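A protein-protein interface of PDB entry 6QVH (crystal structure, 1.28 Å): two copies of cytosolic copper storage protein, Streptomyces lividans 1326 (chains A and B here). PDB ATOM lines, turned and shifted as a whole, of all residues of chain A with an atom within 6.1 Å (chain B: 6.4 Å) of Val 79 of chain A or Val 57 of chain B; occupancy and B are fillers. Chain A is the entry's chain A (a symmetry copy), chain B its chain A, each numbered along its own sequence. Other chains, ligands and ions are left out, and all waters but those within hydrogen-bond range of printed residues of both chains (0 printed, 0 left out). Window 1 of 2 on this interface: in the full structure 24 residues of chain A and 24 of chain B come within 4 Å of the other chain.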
ATOM      1  N   VAL A  57     -28.413 -16.489  15.739  1.00  0.00           N
ATOM      2  CA  VAL A  57     -27.318 -16.636  14.744  1.00  0.00           C
ATOM      3  C   VAL A  57     -26.316 -15.504  14.956  1.00  0.00           C
ATOM      4  O   VAL A  57     -25.102 -15.790  14.925  1.00  0.00           O
ATOM      5  CB  VAL A  57     -27.854 -16.703  13.307  1.00  0.00           C
ATOM      6  CG1 VAL A  57     -26.726 -16.738  12.291  1.00  0.00           C
ATOM      7  CG2 VAL A  57     -28.767 -17.902  13.113  1.00  0.00           C
ATOM      8  N   ALA A  60     -24.086 -16.413  17.954  1.00  0.00           N
ATOM      9  CA  ALA A  60     -23.116 -17.475  17.618  1.00  0.00           C
ATOM     10  C   ALA A  60     -22.020 -16.887  16.726  1.00  0.00           C
ATOM     11  O   ALA A  60     -20.836 -17.229  16.939  1.00  0.00           O
ATOM     12  CB  ALA A  60     -23.821 -18.630  16.951  1.00  0.00           C
ATOM     13  N   THR A  61     -22.387 -16.051  15.754  1.00  0.00           N
ATOM     14  CA  THR A  61     -21.425 -15.484  14.782  1.00  0.00           C
ATOM     15  C   THR A  61     -20.444 -14.579  15.526  1.00  0.00           C
ATOM     16  O   THR A  61     -19.237 -14.635  15.227  1.00  0.00           O
ATOM     17  CB  THR A  61     -22.163 -14.769  13.655  1.00  0.00           C
ATOM     18  OG1 THR A  61     -23.020 -15.709  13.008  1.00  0.00           O
ATOM     19  CG2 THR A  61     -21.205 -14.188  12.638  1.00  0.00           C
ATOM     20  N   VAL A  64     -17.883 -16.885  17.275  1.00  0.00           N
ATOM     21  CA  VAL A  64     -16.966 -17.562  16.318  1.00  0.00           C
ATOM     22  C   VAL A  64     -15.958 -16.533  15.787  1.00  0.00           C
ATOM     23  O   VAL A  64     -14.746 -16.843  15.730  1.00  0.00           O
ATOM     24  CB  VAL A  64     -17.771 -18.241  15.196  1.00  0.00           C
ATOM     25  CG1 VAL A  64     -16.879 -18.681  14.041  1.00  0.00           C
ATOM     26  CG2 VAL A  64     -18.585 -19.402  15.754  1.00  0.00           C
ATOM     27  N   LEU A  65     -16.407 -15.330  15.438  1.00  0.00           N
ATOM     28  CA  LEU A  65     -15.531 -14.319  14.784  1.00  0.00           C
ATOM     29  C   LEU A  65     -14.555 -13.712  15.801  1.00  0.00           C
ATOM     30  O   LEU A  65     -13.501 -13.222  15.393  1.00  0.00           O
ATOM     31  CB  LEU A  65     -16.394 -13.258  14.096  1.00  0.00           C
ATOM     32  CG  LEU A  65     -16.769 -13.556  12.646  1.00  0.00           C
ATOM     33  CD1 LEU A  65     -15.582 -13.354  11.715  1.00  0.00           C
ATOM     34  CD2 LEU A  65     -17.325 -14.964  12.477  1.00  0.00           C
ATOM     35  N   ASN A  74     -13.151 -22.058   6.264  1.00  0.00           N
ATOM     36  CA  ASN A  74     -14.370 -22.793   5.829  1.00  0.00           C
ATOM     37  C   ASN A  74     -15.473 -22.599   6.867  1.00  0.00           C
ATOM     38  O   ASN A  74     -16.613 -22.291   6.478  1.00  0.00           O
ATOM     39  CB  ASN A  74     -14.113 -24.287   5.622  1.00  0.00           C
ATOM     40  CG  ASN A  74     -13.209 -24.559   4.442  1.00  0.00           C
ATOM     41  OD1 ASN A  74     -13.247 -23.831   3.452  1.00  0.00           O
ATOM     42  ND2 ASN A  74     -12.396 -25.600   4.540  1.00  0.00           N
ATOM     43  N   VAL A  75     -15.137 -22.776   8.144  1.00  0.00           N
ATOM     44  CA  VAL A  75     -16.109 -22.598   9.260  1.00  0.00           C
ATOM     45  C   VAL A  75     -16.547 -21.130   9.274  1.00  0.00           C
ATOM     46  O   VAL A  75     -17.748 -20.848   9.269  1.00  0.00           O
ATOM     47  CB  VAL A  75     -15.503 -23.026  10.609  1.00  0.00           C
ATOM     48  CG1 VAL A  75     -16.373 -22.593  11.785  1.00  0.00           C
ATOM     49  CG2 VAL A  75     -15.243 -24.523  10.642  1.00  0.00           C
ATOM     50  N   THR A  76     -15.595 -20.206   9.268  1.00  0.00           N
ATOM     51  CA  THR A  76     -15.888 -18.753   9.368  1.00  0.00           C
ATOM     52  C   THR A  76     -16.758 -18.306   8.184  1.00  0.00           C
ATOM     53  O   THR A  76     -17.758 -17.618   8.426  1.00  0.00           O
ATOM     54  CB  THR A  76     -14.599 -17.945   9.515  1.00  0.00           C
ATOM     55  OG1 THR A  76     -13.983 -18.391  10.725  1.00  0.00           O
ATOM     56  CG2 THR A  76     -14.857 -16.457   9.566  1.00  0.00           C
ATOM     57  N   ARG A  77     -16.418 -18.697   6.952  1.00  0.00           N
ATOM     58  CA  ARG A  77     -17.238 -18.358   5.758  1.00  0.00           C
ATOM     59  C   ARG A  77     -18.673 -18.878   5.941  1.00  0.00           C
ATOM     60  O   ARG A  77     -19.611 -18.107   5.686  1.00  0.00           O
ATOM     61  CB  ARG A  77     -16.630 -18.937   4.475  1.00  0.00           C
ATOM     62  CG  ARG A  77     -15.464 -18.141   3.904  1.00  0.00           C
ATOM     63  CD  ARG A  77     -15.083 -18.609   2.507  1.00  0.00           C
ATOM     64  NE  ARG A  77     -14.411 -19.903   2.534  1.00  0.00           N
ATOM     65  CZ  ARG A  77     -13.095 -20.101   2.453  1.00  0.00           C
ATOM     66  NH1 ARG A  77     -12.255 -19.085   2.325  1.00  0.00           N
ATOM     67  NH2 ARG A  77     -12.619 -21.333   2.500  1.00  0.00           N
ATOM     68  N   ALA A  78     -18.848 -20.149   6.318  1.00  0.00           N
ATOM     69  CA  ALA A  78     -20.179 -20.792   6.446  1.00  0.00           C
ATOM     70  C   ALA A  78     -21.001 -20.062   7.512  1.00  0.00           C
ATOM     71  O   ALA A  78     -22.198 -19.805   7.285  1.00  0.00           O
ATOM     72  CB  ALA A  78     -20.029 -22.263   6.752  1.00  0.00           C
ATOM     73  N   VAL A  79     -20.378 -19.697   8.628  1.00  0.00           N
ATOM     74  CA  VAL A  79     -21.096 -18.984   9.726  1.00  0.00           C
ATOM     75  C   VAL A  79     -21.482 -17.578   9.243  1.00  0.00           C
ATOM     76  O   VAL A  79     -22.630 -17.178   9.444  1.00  0.00           O
ATOM     77  CB  VAL A  79     -20.257 -18.988  11.011  1.00  0.00           C
ATOM     78  CG1 VAL A  79     -20.849 -18.104  12.088  1.00  0.00           C
ATOM     79  CG2 VAL A  79     -20.072 -20.405  11.529  1.00  0.00           C
ATOM     80  N   LEU A  80     -20.580 -16.863   8.568  1.00  0.00           N
ATOM     81  CA  LEU A  80     -20.880 -15.508   8.040  1.00  0.00           C
ATOM     82  C   LEU A  80     -22.005 -15.586   7.007  1.00  0.00           C
ATOM     83  O   LEU A  80     -22.869 -14.700   7.001  1.00  0.00           O
ATOM     84  CB  LEU A  80     -19.612 -14.907   7.428  1.00  0.00           C
ATOM     85  CG  LEU A  80     -18.564 -14.455   8.443  1.00  0.00           C
ATOM     86  CD1 LEU A  80     -17.268 -14.093   7.741  1.00  0.00           C
ATOM     87  CD2 LEU A  80     -19.069 -13.278   9.270  1.00  0.00           C
ATOM     88  N   GLN A  81     -22.003 -16.612   6.160  1.00  0.00           N
ATOM     89  CA  GLN A  81     -23.072 -16.771   5.142  1.00  0.00           C
ATOM     90  C   GLN A  81     -24.407 -16.952   5.867  1.00  0.00           C
ATOM     91  O   GLN A  81     -25.401 -16.311   5.471  1.00  0.00           O
ATOM     92  CB  GLN A  81     -22.813 -17.941   4.192  1.00  0.00           C
ATOM     93  CG  GLN A  81     -23.840 -18.018   3.070  1.00  0.00           C
ATOM     94  CD  GLN A  81     -24.016 -16.714   2.322  1.00  0.00           C
ATOM     95  OE1 GLN A  81     -25.043 -16.041   2.418  1.00  0.00           O
ATOM     96  NE2 GLN A  81     -23.003 -16.338   1.563  1.00  0.00           N
ATOM     97  N   ALA A  82     -24.434 -17.772   6.915  1.00  0.00           N
ATOM     98  CA  ALA A  82     -25.681 -17.989   7.682  1.00  0.00           C
ATOM     99  C   ALA A  82     -26.132 -16.657   8.276  1.00  0.00           C
ATOM    100  O   ALA A  82     -27.319 -16.318   8.198  1.00  0.00           O
ATOM    101  CB  ALA A  82     -25.506 -19.036   8.747  1.00  0.00           C
ATOM    102  N   CYS A  83     -25.209 -15.903   8.860  1.00  0.00           N
ATOM    103  CA  CYS A  83     -25.611 -14.650   9.529  1.00  0.00           C
ATOM    104  C   CYS A  83     -26.079 -13.624   8.496  1.00  0.00           C
ATOM    105  O   CYS A  83     -27.047 -12.884   8.774  1.00  0.00           O
ATOM    106  CB  CYS A  83     -24.512 -14.069  10.398  1.00  0.00           C
ATOM    107  SG  CYS A  83     -25.245 -13.101  11.741  1.00  0.00           S
ATOM    108  N   ALA A  84     -25.412 -13.551   7.349  1.00  0.00           N
ATOM    109  CA  ALA A  84     -25.816 -12.622   6.274  1.00  0.00           C
ATOM    110  C   ALA A  84     -27.249 -12.952   5.852  1.00  0.00           C
ATOM    111  O   ALA A  84     -28.090 -12.033   5.748  1.00  0.00           O
ATOM    112  CB  ALA A  84     -24.864 -12.708   5.109  1.00  0.00           C
ATOM    113  N   CYS B  21     -28.010 -31.901  17.502  1.00  0.00           N
ATOM    114  CA  CYS B  21     -27.402 -30.574  17.768  1.00  0.00           C
ATOM    115  C   CYS B  21     -27.232 -30.405  19.281  1.00  0.00           C
ATOM    116  O   CYS B  21     -26.167 -29.964  19.711  1.00  0.00           O
ATOM    117  CB  CYS B  21     -28.221 -29.406  17.235  1.00  0.00           C
ATOM    118  SG  CYS B  21     -28.109 -29.145  15.442  1.00  0.00           S
ATOM    119  N   MET B  52     -15.499 -24.983  20.968  1.00  0.00           N
ATOM    120  CA  MET B  52     -16.299 -23.792  21.365  1.00  0.00           C
ATOM    121  C   MET B  52     -17.162 -23.343  20.185  1.00  0.00           C
ATOM    122  O   MET B  52     -18.371 -23.095  20.392  1.00  0.00           O
ATOM    123  CB  MET B  52     -15.411 -22.651  21.850  1.00  0.00           C
ATOM    124  CG  MET B  52     -14.723 -23.008  23.148  1.00  0.00           C
ATOM    125  SD  MET B  52     -14.010 -21.573  23.896  1.00  0.00           S
ATOM    126  CE  MET B  52     -12.866 -21.196  22.593  1.00  0.00           C
ATOM    127  N   ASP B  53     -16.599 -23.255  18.980  1.00  0.00           N
ATOM    128  CA  ASP B  53     -17.387 -22.837  17.790  1.00  0.00           C
ATOM    129  C   ASP B  53     -18.506 -23.853  17.580  1.00  0.00           C
ATOM    130  O   ASP B  53     -19.639 -23.483  17.269  1.00  0.00           O
ATOM    131  CB  ASP B  53     -16.546 -22.808  16.516  1.00  0.00           C
ATOM    132  CG  ASP B  53     -15.539 -21.684  16.431  1.00  0.00           C
ATOM    133  OD1 ASP B  53     -15.615 -20.747  17.251  1.00  0.00           O
ATOM    134  OD2 ASP B  53     -14.687 -21.751  15.528  1.00  0.00           O
ATOM    135  N   CYS B  54     -18.164 -25.126  17.659  1.00  0.00           N
ATOM    136  CA  CYS B  54     -19.123 -26.187  17.309  1.00  0.00           C
ATOM    137  C   CYS B  54     -20.277 -26.193  18.307  1.00  0.00           C
ATOM    138  O   CYS B  54     -21.419 -26.421  17.884  1.00  0.00           O
ATOM    139  CB  CYS B  54     -18.444 -27.539  17.248  1.00  0.00           C
ATOM    140  SG  CYS B  54     -19.364 -28.691  16.213  1.00  0.00           S
ATOM    141  N   ALA B  55     -20.008 -25.929  19.583  1.00  0.00           N
ATOM    142  CA  ALA B  55     -21.067 -25.840  20.607  1.00  0.00           C
ATOM    143  C   ALA B  55     -21.956 -24.634  20.278  1.00  0.00           C
ATOM    144  O   ALA B  55     -23.186 -24.746  20.344  1.00  0.00           O
ATOM    145  CB  ALA B  55     -20.488 -25.723  21.991  1.00  0.00           C
ATOM    146  N   ASP B  56     -21.365 -23.494  19.926  1.00  0.00           N
ATOM    147  CA  ASP B  56     -22.144 -22.247  19.693  1.00  0.00           C
ATOM    148  C   ASP B  56     -23.061 -22.459  18.487  1.00  0.00           C
ATOM    149  O   ASP B  56     -24.241 -22.089  18.542  1.00  0.00           O
ATOM    150  CB  ASP B  56     -21.225 -21.044  19.497  1.00  0.00           C
ATOM    151  CG  ASP B  56     -20.534 -20.616  20.774  1.00  0.00           C
ATOM    152  OD1 ASP B  56     -21.000 -21.019  21.856  1.00  0.00           O
ATOM    153  OD2 ASP B  56     -19.502 -19.971  20.658  1.00  0.00           O
ATOM    154  N   VAL B  57     -22.552 -23.068  17.427  1.00  0.00           N
ATOM    155  CA  VAL B  57     -23.332 -23.218  16.170  1.00  0.00           C
ATOM    156  C   VAL B  57     -24.394 -24.294  16.386  1.00  0.00           C
ATOM    157  O   VAL B  57     -25.544 -24.069  15.958  1.00  0.00           O
ATOM    158  CB  VAL B  57     -22.428 -23.501  14.963  1.00  0.00           C
ATOM    159  CG1 VAL B  57     -23.238 -23.767  13.707  1.00  0.00           C
ATOM    160  CG2 VAL B  57     -21.454 -22.359  14.723  1.00  0.00           C
ATOM    161  N   CYS B  58     -24.071 -25.401  17.055  1.00  0.00           N
ATOM    162  CA  CYS B  58     -25.083 -26.463  17.305  1.00  0.00           C
ATOM    163  C   CYS B  58     -26.213 -25.882  18.171  1.00  0.00           C
ATOM    164  O   CYS B  58     -27.402 -26.172  17.910  1.00  0.00           O
ATOM    165  CB  CYS B  58     -24.475 -27.698  17.965  1.00  0.00           C
ATOM    166  SG  CYS B  58     -23.551 -28.759  16.824  1.00  0.00           S
ATOM    167  N   THR B  59     -25.883 -25.048  19.161  1.00  0.00           N
ATOM    168  CA  THR B  59     -26.903 -24.432  20.049  1.00  0.00           C
ATOM    169  C   THR B  59     -27.855 -23.584  19.199  1.00  0.00           C
ATOM    170  O   THR B  59     -29.097 -23.715  19.330  1.00  0.00           O
ATOM    171  CB  THR B  59     -26.227 -23.637  21.177  1.00  0.00           C
ATOM    172  OG1 THR B  59     -25.527 -24.573  21.996  1.00  0.00           O
ATOM    173  CG2 THR B  59     -27.202 -22.859  22.032  1.00  0.00           C
ATOM    174  N   ALA B  60     -27.315 -22.731  18.338  1.00  0.00           N
ATOM    175  CA  ALA B  60     -28.120 -21.825  17.494  1.00  0.00           C
ATOM    176  C   ALA B  60     -28.956 -22.659  16.521  1.00  0.00           C
ATOM    177  O   ALA B  60     -30.141 -22.317  16.313  1.00  0.00           O
ATOM    178  CB  ALA B  60     -27.221 -20.854  16.770  1.00  0.00           C
ATOM    179  N   THR B  61     -28.371 -23.702  15.930  1.00  0.00           N
ATOM    180  CA  THR B  61     -29.055 -24.531  14.913  1.00  0.00           C
ATOM    181  C   THR B  61     -30.231 -25.251  15.571  1.00  0.00           C
ATOM    182  O   THR B  61     -31.310 -25.317  14.953  1.00  0.00           O
ATOM    183  CB  THR B  61     -28.066 -25.483  14.247  1.00  0.00           C
ATOM    184  OG1 THR B  61     -27.034 -24.710  13.637  1.00  0.00           O
ATOM    185  CG2 THR B  61     -28.736 -26.339  13.193  1.00  0.00           C
ATOM    186  N   ALA B  62     -30.047 -25.779  16.775  1.00  0.00           N
ATOM    187  CA  ALA B  62     -31.125 -26.508  17.482  1.00  0.00           C
ATOM    188  C   ALA B  62     -32.316 -25.568  17.668  1.00  0.00           C
ATOM    189  O   ALA B  62     -33.458 -26.014  17.501  1.00  0.00           O
ATOM    190  CB  ALA B  62     -30.644 -27.025  18.812  1.00  0.00           C
ATOM    191  N   VAL B  79     -28.256 -22.067   7.841  1.00  0.00           N
ATOM    192  CA  VAL B  79     -27.886 -22.450   9.236  1.00  0.00           C
ATOM    193  C   VAL B  79     -27.435 -23.918   9.250  1.00  0.00           C
ATOM    194  O   VAL B  79     -26.398 -24.213   9.848  1.00  0.00           O
ATOM    195  CB  VAL B  79     -29.039 -22.149  10.203  1.00  0.00           C
ATOM    196  CG1 VAL B  79     -28.790 -22.708  11.588  1.00  0.00           C
ATOM    197  CG2 VAL B  79     -29.306 -20.654  10.273  1.00  0.00           C
ATOM    198  N   ALA B  82     -23.960 -24.219   7.833  1.00  0.00           N
ATOM    199  CA  ALA B  82     -22.959 -23.770   8.826  1.00  0.00           C
ATOM    200  C   ALA B  82     -22.732 -24.889   9.839  1.00  0.00           C
ATOM    201  O   ALA B  82     -21.581 -25.195  10.172  1.00  0.00           O
ATOM    202  CB  ALA B  82     -23.376 -22.493   9.501  1.00  0.00           C
ATOM    203  N   CYS B  83     -23.804 -25.502  10.325  1.00  0.00           N
ATOM    204  CA  CYS B  83     -23.642 -26.528  11.374  1.00  0.00           C
ATOM    205  C   CYS B  83     -22.950 -27.766  10.802  1.00  0.00           C
ATOM    206  O   CYS B  83     -22.119 -28.376  11.509  1.00  0.00           O
ATOM    207  CB  CYS B  83     -24.954 -26.907  12.033  1.00  0.00           C
ATOM    208  SG  CYS B  83     -24.645 -27.474  13.725  1.00  0.00           S
ATOM    209  N   ALA B  84     -23.285 -28.153   9.576  1.00  0.00           N
ATOM    210  CA  ALA B  84     -22.641 -29.311   8.923  1.00  0.00           C
ATOM    211  C   ALA B  84     -21.136 -29.048   8.833  1.00  0.00           C
ATOM    212  O   ALA B  84     -20.331 -29.932   9.197  1.00  0.00           O
ATOM    213  CB  ALA B  84     -23.240 -29.558   7.563  1.00  0.00           C
ATOM    214  N   VAL B  86     -19.136 -26.901  10.528  1.00  0.00           N
ATOM    215  CA  VAL B  86     -18.349 -26.844  11.791  1.00  0.00           C
ATOM    216  C   VAL B  86     -18.276 -28.249  12.410  1.00  0.00           C
ATOM    217  O   VAL B  86     -17.220 -28.604  12.950  1.00  0.00           O
ATOM    218  CB  VAL B  86     -18.876 -25.782  12.770  1.00  0.00           C
ATOM    219  CG1 VAL B  86     -20.252 -26.120  13.305  1.00  0.00           C
ATOM    220  CG2 VAL B  86     -17.902 -25.554  13.912  1.00  0.00           C
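Among the printed residues, pairs that only touch across the chains: Val 57 of chain A with Val 79 of chain B (3.99 Å), Ala 60 of chain A with Asp 56 of chain B (3.8 Å), Val 64 of chain A with Asp 53 of chain B (3.6 Å), Val 75 of chain A with Val 86 of chain B (3.95 Å), Ala 78 of chain A with Ala 82 of chain B (3.7 Å) and Val 79 of chain A with Val 57 of chain B (3.99 Å).
Val 57 of chain A touches Val 79 of chain B, and with the chains exchanged Val 79 of chain A touches Val 57 of chain B. Of the 6 pairs that touch across the chains among the printed residues, 2 have their exchanged pair printed and touching as well.
Hydrophobic or aromatic side chains of chain B that line the printed part of chain A: Val 57, Val 79, Ala 82 and Val 86. Hydrophobic or aromatic side chains of chain A that line the printed part of chain B: Val 57, Ala 60, Val 64, Val 75, Ala 78 and Val 79. Among the printed residues, 6 pairs touch across the chains.
The backbone carbonyl oxygen (O) of Val 57 of chain B lies within hydrogen-bond range of the side-chain hydroxyl (OG1) of Thr 61 of chain B, 2.8 Å away. OG1 of Thr 61 of chain A lies within hydrogen-bond range of O of Val 57 of chain A, 2.8 Å away.
Of the printed residues of chain B, Val 79 of chain A touches Val 57 (3.99 Å). Of the printed residues of chain A, Val 57 of chain B touches Val 79. Of the printed residues of chain A, Ala 82 of chain B touches Ala 78 (3.7 Å). Printed residues of chain A within 4 Å of Val 86 of chain B: Val 75. Thr 61 of chain B touches none of the printed residues of chain A. The nearest printed residue of chain B that does not touch Val 79 of chain A is Ala 82 of chain B (4.2 Å).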
